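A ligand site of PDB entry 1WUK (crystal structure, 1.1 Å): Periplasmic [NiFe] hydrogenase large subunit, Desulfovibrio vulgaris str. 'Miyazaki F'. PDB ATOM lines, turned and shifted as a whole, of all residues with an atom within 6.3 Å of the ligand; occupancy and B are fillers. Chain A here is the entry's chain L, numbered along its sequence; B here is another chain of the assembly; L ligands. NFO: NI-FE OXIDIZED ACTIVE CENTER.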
ATOM      1  N   GLU A  16       6.969   9.698   1.084  1.00  0.00           N
ATOM      2  CA  GLU A  16       5.742  10.486   1.223  1.00  0.00           C
ATOM      3  C   GLU A  16       4.603   9.487   0.963  1.00  0.00           C
ATOM      4  O   GLU A  16       4.551   8.776  -0.036  1.00  0.00           O
ATOM      5  CB  GLU A  16       5.686  11.618   0.211  1.00  0.00           C
ATOM      6  CG  GLU A  16       4.567  12.622   0.476  1.00  0.00           C
ATOM      7  CD  GLU A  16       3.156  12.093   0.291  1.00  0.00           C
ATOM      8  OE1 GLU A  16       2.238  12.439   1.056  1.00  0.00           O
ATOM      9  OE2 GLU A  16       3.006  11.233  -0.619  1.00  0.00           O
ATOM     10  N   THR A  62      -1.403  18.333  -4.392  1.00  0.00           N
ATOM     11  CA  THR A  62      -1.081  16.932  -4.646  1.00  0.00           C
ATOM     12  C   THR A  62       0.032  16.494  -3.704  1.00  0.00           C
ATOM     13  O   THR A  62       0.030  15.358  -3.220  1.00  0.00           O
ATOM     14  CB  THR A  62      -0.631  16.734  -6.089  1.00  0.00           C
ATOM     15  OG1 THR A  62      -1.720  17.039  -6.989  1.00  0.00           O
ATOM     16  CG2 THR A  62      -0.212  15.308  -6.341  1.00  0.00           C
ATOM     17  N   CYS A  63       1.007  17.395  -3.439  1.00  0.00           N
ATOM     18  CA  CYS A  63       2.195  16.975  -2.695  1.00  0.00           C
ATOM     19  C   CYS A  63       2.948  18.174  -2.135  1.00  0.00           C
ATOM     20  O   CYS A  63       3.217  19.119  -2.869  1.00  0.00           O
ATOM     21  CB  CYS A  63       3.105  16.193  -3.605  1.00  0.00           C
ATOM     22  SG  CYS A  63       4.499  15.454  -2.675  1.00  0.00           S
ATOM     23  N   GLY A  64       3.275  18.069  -0.866  1.00  0.00           N
ATOM     24  CA  GLY A  64       4.076  19.091  -0.173  1.00  0.00           C
ATOM     25  C   GLY A  64       5.538  18.769  -0.029  1.00  0.00           C
ATOM     26  O   GLY A  64       6.269  19.614   0.478  1.00  0.00           O
ATOM     27  N   VAL A  65       5.944  17.555  -0.415  1.00  0.00           N
ATOM     28  CA  VAL A  65       7.345  17.185  -0.515  1.00  0.00           C
ATOM     29  C   VAL A  65       7.889  17.780  -1.811  1.00  0.00           C
ATOM     30  O   VAL A  65       8.768  18.655  -1.798  1.00  0.00           O
ATOM     31  CB  VAL A  65       7.551  15.693  -0.389  1.00  0.00           C
ATOM     32  CG1 VAL A  65       9.002  15.315  -0.569  1.00  0.00           C
ATOM     33  CG2 VAL A  65       7.065  15.181   0.971  1.00  0.00           C
ATOM     34  N   CYS A  66       7.320  17.335  -2.950  1.00  0.00           N
ATOM     35  CA  CYS A  66       7.545  17.987  -4.237  1.00  0.00           C
ATOM     36  C   CYS A  66       6.613  19.180  -4.376  1.00  0.00           C
ATOM     37  O   CYS A  66       5.900  19.343  -5.355  1.00  0.00           O
ATOM     38  CB  CYS A  66       7.473  16.993  -5.374  1.00  0.00           C
ATOM     39  SG  CYS A  66       5.863  16.239  -5.672  1.00  0.00           S
ATOM     40  N   THR A  67       6.615  20.019  -3.349  1.00  0.00           N
ATOM     41  CA  THR A  67       5.880  21.277  -3.432  1.00  0.00           C
ATOM     42  C   THR A  67       6.426  22.063  -4.625  1.00  0.00           C
ATOM     43  O   THR A  67       7.479  21.778  -5.189  1.00  0.00           O
ATOM     44  CB  THR A  67       6.025  22.046  -2.100  1.00  0.00           C
ATOM     45  OG1 THR A  67       5.112  23.115  -2.141  1.00  0.00           O
ATOM     46  CG2 THR A  67       7.420  22.586  -1.883  1.00  0.00           C
ATOM     47  N   THR A  69       6.171  21.906  -7.683  1.00  0.00           N
ATOM     48  CA  THR A  69       6.209  21.216  -8.949  1.00  0.00           C
ATOM     49  C   THR A  69       4.848  21.129  -9.636  1.00  0.00           C
ATOM     50  O   THR A  69       4.775  21.323 -10.861  1.00  0.00           O
ATOM     51  CB  THR A  69       6.839  19.817  -8.846  1.00  0.00           C
ATOM     52  OG1 THR A  69       6.017  18.921  -8.131  1.00  0.00           O
ATOM     53  CG2 THR A  69       8.225  19.863  -8.236  1.00  0.00           C
ATOM     54  N   HIS A  70       3.781  20.839  -8.888  1.00  0.00           N
ATOM     55  CA  HIS A  70       2.451  20.727  -9.509  1.00  0.00           C
ATOM     56  C   HIS A  70       1.877  22.092  -9.830  1.00  0.00           C
ATOM     57  O   HIS A  70       1.121  22.218 -10.808  1.00  0.00           O
ATOM     58  CB  HIS A  70       1.538  19.906  -8.630  1.00  0.00           C
ATOM     59  CG  HIS A  70       1.846  18.452  -8.592  1.00  0.00           C
ATOM     60  ND1 HIS A  70       1.446  17.579  -9.546  1.00  0.00           N
ATOM     61  CD2 HIS A  70       2.575  17.793  -7.643  1.00  0.00           C
ATOM     62  CE1 HIS A  70       1.912  16.404  -9.164  1.00  0.00           C
ATOM     63  NE2 HIS A  70       2.601  16.478  -8.014  1.00  0.00           N
ATOM     64  N   ASP A 105      14.921  18.866  -2.045  1.00  0.00           N
ATOM     65  CA  ASP A 105      14.237  17.560  -2.056  1.00  0.00           C
ATOM     66  C   ASP A 105      15.282  16.445  -2.005  1.00  0.00           C
ATOM     67  O   ASP A 105      15.196  15.528  -1.202  1.00  0.00           O
ATOM     68  CB  ASP A 105      13.354  17.532  -3.332  1.00  0.00           C
ATOM     69  CG  ASP A 105      12.232  16.535  -3.315  1.00  0.00           C
ATOM     70  OD1 ASP A 105      12.360  15.477  -2.620  1.00  0.00           O
ATOM     71  OD2 ASP A 105      11.229  16.759  -4.045  1.00  0.00           O
ATOM     72  N   ALA A 459      10.329  16.762 -12.585  1.00  0.00           N
ATOM     73  CA  ALA A 459      10.383  17.010 -11.161  1.00  0.00           C
ATOM     74  C   ALA A 459      11.463  16.172 -10.520  1.00  0.00           C
ATOM     75  O   ALA A 459      12.080  15.339 -11.218  1.00  0.00           O
ATOM     76  CB  ALA A 459       8.992  16.661 -10.565  1.00  0.00           C
ATOM     77  N   PRO A 460      11.726  16.313  -9.239  1.00  0.00           N
ATOM     78  CA  PRO A 460      12.775  15.483  -8.602  1.00  0.00           C
ATOM     79  C   PRO A 460      12.595  13.983  -8.747  1.00  0.00           C
ATOM     80  O   PRO A 460      13.600  13.245  -8.684  1.00  0.00           O
ATOM     81  CB  PRO A 460      12.745  15.960  -7.130  1.00  0.00           C
ATOM     82  CG  PRO A 460      12.329  17.430  -7.270  1.00  0.00           C
ATOM     83  CD  PRO A 460      11.259  17.369  -8.317  1.00  0.00           C
ATOM     84  N   ARG A 461      11.369  13.504  -8.933  1.00  0.00           N
ATOM     85  CA  ARG A 461      11.096  12.078  -9.131  1.00  0.00           C
ATOM     86  C   ARG A 461      10.826  11.701 -10.579  1.00  0.00           C
ATOM     87  O   ARG A 461      10.606  10.538 -10.870  1.00  0.00           O
ATOM     88  CB  ARG A 461       9.979  11.617  -8.206  1.00  0.00           C
ATOM     89  CG  ARG A 461      10.376  11.728  -6.736  1.00  0.00           C
ATOM     90  CD  ARG A 461       9.154  11.755  -5.805  1.00  0.00           C
ATOM     91  NE  ARG A 461       9.632  12.009  -4.439  1.00  0.00           N
ATOM     92  CZ  ARG A 461      10.065  13.167  -3.983  1.00  0.00           C
ATOM     93  NH1 ARG A 461       9.904  14.289  -4.694  1.00  0.00           N
ATOM     94  NH2 ARG A 461      10.605  13.243  -2.786  1.00  0.00           N
ATOM     95  N   GLY A 462      10.858  12.677 -11.508  1.00  0.00           N
ATOM     96  CA  GLY A 462      10.800  12.399 -12.927  1.00  0.00           C
ATOM     97  C   GLY A 462       9.698  13.138 -13.669  1.00  0.00           C
ATOM     98  O   GLY A 462       9.296  14.257 -13.323  1.00  0.00           O
ATOM     99  N   GLY A 463       9.223  12.513 -14.742  1.00  0.00           N
ATOM    100  CA  GLY A 463       8.374  13.217 -15.714  1.00  0.00           C
ATOM    101  C   GLY A 463       6.942  13.390 -15.227  1.00  0.00           C
ATOM    102  O   GLY A 463       6.177  12.415 -15.120  1.00  0.00           O
ATOM    103  N   LEU A 464       6.580  14.638 -14.965  1.00  0.00           N
ATOM    104  CA  LEU A 464       5.275  15.099 -14.522  1.00  0.00           C
ATOM    105  C   LEU A 464       4.571  15.771 -15.680  1.00  0.00           C
ATOM    106  O   LEU A 464       5.107  16.637 -16.339  1.00  0.00           O
ATOM    107  CB  LEU A 464       5.440  16.084 -13.372  1.00  0.00           C
ATOM    108  CG  LEU A 464       4.200  16.805 -12.903  1.00  0.00           C
ATOM    109  CD1 LEU A 464       3.124  15.843 -12.409  1.00  0.00           C
ATOM    110  CD2 LEU A 464       4.547  17.823 -11.802  1.00  0.00           C
ATOM    111  N   VAL A 482       1.796  11.378 -12.953  1.00  0.00           N
ATOM    112  CA  VAL A 482       2.821  11.894 -12.046  1.00  0.00           C
ATOM    113  C   VAL A 482       3.983  10.914 -12.020  1.00  0.00           C
ATOM    114  O   VAL A 482       3.810   9.730 -12.316  1.00  0.00           O
ATOM    115  CB  VAL A 482       2.147  12.162 -10.686  1.00  0.00           C
ATOM    116  CG1 VAL A 482       3.060  12.830  -9.683  1.00  0.00           C
ATOM    117  CG2 VAL A 482       0.950  13.039 -10.886  1.00  0.00           C
ATOM    118  N   PRO A 483       5.229  11.358 -11.739  1.00  0.00           N
ATOM    119  CA  PRO A 483       6.367  10.438 -11.828  1.00  0.00           C
ATOM    120  C   PRO A 483       6.179   9.145 -11.042  1.00  0.00           C
ATOM    121  O   PRO A 483       6.425   8.050 -11.556  1.00  0.00           O
ATOM    122  CB  PRO A 483       7.567  11.270 -11.371  1.00  0.00           C
ATOM    123  CG  PRO A 483       7.123  12.650 -11.317  1.00  0.00           C
ATOM    124  CD  PRO A 483       5.710  12.738 -11.572  1.00  0.00           C
ATOM    125  N   SER A 484       5.743   9.254  -9.790  1.00  0.00           N
ATOM    126  CA  SER A 484       5.565   8.048  -8.982  1.00  0.00           C
ATOM    127  C   SER A 484       4.436   7.160  -9.529  1.00  0.00           C
ATOM    128  O   SER A 484       4.433   5.961  -9.244  1.00  0.00           O
ATOM    129  CB  SER A 484       5.311   8.381  -7.531  1.00  0.00           C
ATOM    130  OG  SER A 484       6.433   8.933  -6.894  1.00  0.00           O
ATOM    131  N   THR A 485       3.497   7.736 -10.329  1.00  0.00           N
ATOM    132  CA  THR A 485       2.522   6.891 -10.989  1.00  0.00           C
ATOM    133  C   THR A 485       3.236   5.948 -11.959  1.00  0.00           C
ATOM    134  O   THR A 485       2.947   4.737 -12.025  1.00  0.00           O
ATOM    135  CB  THR A 485       1.447   7.750 -11.750  1.00  0.00           C
ATOM    136  OG1 THR A 485       1.094   8.926 -11.031  1.00  0.00           O
ATOM    137  CG2 THR A 485       0.211   6.906 -11.985  1.00  0.00           C
ATOM    138  N   ASP A 526      12.519   6.888  -4.489  1.00  0.00           N
ATOM    139  CA  ASP A 526      11.959   8.093  -3.824  1.00  0.00           C
ATOM    140  C   ASP A 526      10.440   8.173  -4.018  1.00  0.00           C
ATOM    141  O   ASP A 526       9.914   9.095  -4.636  1.00  0.00           O
ATOM    142  CB  ASP A 526      12.696   9.303  -4.325  1.00  0.00           C
ATOM    143  CG  ASP A 526      12.412  10.627  -3.706  1.00  0.00           C
ATOM    144  OD1 ASP A 526      12.922  11.635  -4.292  1.00  0.00           O
ATOM    145  OD2 ASP A 526      11.731  10.668  -2.653  1.00  0.00           O
ATOM    146  N   PRO A 527       9.708   7.182  -3.527  1.00  0.00           N
ATOM    147  CA  PRO A 527       8.255   7.157  -3.759  1.00  0.00           C
ATOM    148  C   PRO A 527       7.530   8.346  -3.154  1.00  0.00           C
ATOM    149  O   PRO A 527       7.775   8.770  -2.021  1.00  0.00           O
ATOM    150  CB  PRO A 527       7.795   5.867  -3.049  1.00  0.00           C
ATOM    151  CG  PRO A 527       9.035   5.027  -2.960  1.00  0.00           C
ATOM    152  CD  PRO A 527      10.140   6.010  -2.744  1.00  0.00           C
ATOM    153  N   CSO A 528       6.508   8.796  -3.876  1.00  0.00           N
ATOM    154  CA  CSO A 528       5.616   9.853  -3.398  1.00  0.00           C
ATOM    155  CB  CSO A 528       6.023  11.173  -4.047  1.00  0.00           C
ATOM    156  SG  CSO A 528       5.423  12.592  -3.201  1.00  0.00           S
ATOM    157  C   CSO A 528       4.203   9.404  -3.757  1.00  0.00           C
ATOM    158  O   CSO A 528       3.795   9.459  -4.910  1.00  0.00           O
ATOM    159  OD  CSO A 528       4.014  12.326  -2.970  1.00  0.00           O
ATOM    160  N   ILE A 529       3.471   8.892  -2.768  1.00  0.00           N
ATOM    161  CA  ILE A 529       2.202   8.222  -3.054  1.00  0.00           C
ATOM    162  C   ILE A 529       1.057   9.216  -3.203  1.00  0.00           C
ATOM    163  O   ILE A 529       0.104   8.980  -3.965  1.00  0.00           O
ATOM    164  CB  ILE A 529       1.907   7.172  -1.991  1.00  0.00           C
ATOM    165  CG1 ILE A 529       3.085   6.262  -1.716  1.00  0.00           C
ATOM    166  CG2 ILE A 529       0.646   6.358  -2.373  1.00  0.00           C
ATOM    167  CD1 ILE A 529       3.645   5.559  -2.937  1.00  0.00           C
ATOM    168  N   ALA A 530       1.114  10.352  -2.500  1.00  0.00           N
ATOM    169  CA  ALA A 530       0.171  11.443  -2.729  1.00  0.00           C
ATOM    170  C   ALA A 530       0.286  11.900  -4.175  1.00  0.00           C
ATOM    171  O   ALA A 530      -0.717  12.110  -4.866  1.00  0.00           O
ATOM    172  CB  ALA A 530       0.419  12.581  -1.735  1.00  0.00           C
ATOM    173  N   CYS A 531       1.501  12.027  -4.679  1.00  0.00           N
ATOM    174  CA  CYS A 531       1.778  12.289  -6.084  1.00  0.00           C
ATOM    175  C   CYS A 531       1.208  11.216  -6.956  1.00  0.00           C
ATOM    176  O   CYS A 531       0.516  11.483  -7.952  1.00  0.00           O
ATOM    177  CB  CYS A 531       3.306  12.391  -6.335  1.00  0.00           C
ATOM    178  SG  CYS A 531       3.882  14.106  -6.203  1.00  0.00           S
ATOM    179  N   GLY A 532       1.514   9.961  -6.666  1.00  0.00           N
ATOM    180  CA  GLY A 532       1.182   8.907  -7.599  1.00  0.00           C
ATOM    181  C   GLY A 532      -0.329   8.753  -7.792  1.00  0.00           C
ATOM    182  O   GLY A 532      -0.764   8.442  -8.911  1.00  0.00           O
ATOM    183  N   CYS B  17      -0.996  15.692   2.074  1.00  0.00           N
ATOM    184  CA  CYS B  17       0.013  15.843   1.033  1.00  0.00           C
ATOM    185  C   CYS B  17       1.447  15.874   1.595  1.00  0.00           C
ATOM    186  O   CYS B  17       2.398  16.003   0.819  1.00  0.00           O
ATOM    187  CB  CYS B  17      -0.232  17.111   0.220  1.00  0.00           C
ATOM    188  SG  CYS B  17       0.314  18.672   0.984  1.00  0.00           S
HETATM  189 NI   NFO L   1       5.568  14.416  -4.330  1.00  0.00          NI
HETATM  190 FE   NFO L   1       6.071  14.375  -6.947  1.00  0.00          FE
HETATM  191  C3  NFO L   1       5.673  15.008  -8.474  1.00  0.00           C
HETATM  192  C2  NFO L   1       7.913  14.673  -7.399  1.00  0.00           C
HETATM  193  O3  NFO L   1       5.451  15.415  -9.561  1.00  0.00           O
HETATM  194  N2  NFO L   1       9.026  14.850  -7.672  1.00  0.00           N
HETATM  195  O1  NFO L   1       6.174  11.479  -7.880  1.00  0.00           O
HETATM  196  C1  NFO L   1       6.163  12.599  -7.544  1.00  0.00           C
HETATM  197  O4  NFO L   1       6.708  13.654  -5.216  1.00  0.00           O
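A ring nitrogen (NE2) of His 70 is in hydrogen-bond range of an oxygen (O3) of the ligand (3.4 Å). SG of CSO 528 is bound to NI of the ligand (2.2 Å). A nitrogen (N2) of the ligand lies within hydrogen-bond range of the backbone NH (N) of Arg 461, at 3.0 Å. SG of Cys 531 is bound to FE of the ligand, 2.3 Å away. The backbone NH of Ser 484 is in hydrogen-bond range of an oxygen (O1) of the ligand, 3.0 Å away. The side-chain hydroxyl (OG) of Ser 484 lies within hydrogen-bond range of an oxygen (O1) of the ligand (2.7 Å). The side-chain sulfur of Cys 66 binds an iron atom (FE) of the ligand (2.3 Å). SG of Cys 63 binds NI of the ligand, 2.2 Å away. A nitrogen (N2) of the ligand lies within hydrogen-bond range of the guanidinium group (NH1) of Arg 461, 3.2 Å away.
The side-chain carboxylate of Asp 526 is in salt-bridge range of the guanidinium group of Arg 461, 2.8 Å away. The side-chain sulfur (SG) of Cys 63 lies close to the backbone NH (N) of Val 65. SG of Cys 531 sits close to NE2 of His 70 (3.2 Å). The backbone carbonyl oxygen (O) of Val 482 lies within hydrogen-bond range of the side-chain hydroxyl (OG1) of Thr 485 (3.1 Å). OE2 of Glu 16 sits at hydrogen-bond distance from OD of CSO 528 (2.8 Å). The backbone carbonyl oxygen (O) of Cys 66 lies within hydrogen-bond range of the side-chain hydroxyl (OG1) of Thr 69, 2.8 Å away. N of CSO 528 sits at hydrogen-bond distance from OG of Ser 484, at 3.0 Å. NH2 of Arg 461 lies within salt-bridge range of OD1 of Asp 105, at 2.8 Å.
The backbone nitrogen (N) of Pro 460 sits close to a nitrogen (N2) of the ligand, 3.4 Å away. Merely in contact with the ligand: Pro 483 (3.4 Å), Leu 464 (3.4 Å), Ala 459 (3.4 Å), Val 482 (3.5 Å) and Thr 69 (3.8 Å). Hydrophobic or aromatic side chains within 4 Å of the ligand: His 70, Ala 459, Pro 460, Leu 464, Val 482 and Pro 483. 13 residues have an atom within 4 Å of the ligand: Cys 63, Cys 66, Thr 69, His 70, Ala 459, Pro 460, Arg 461, Leu 464, Val 482, Pro 483, Ser 484, CSO 528 and Cys 531.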
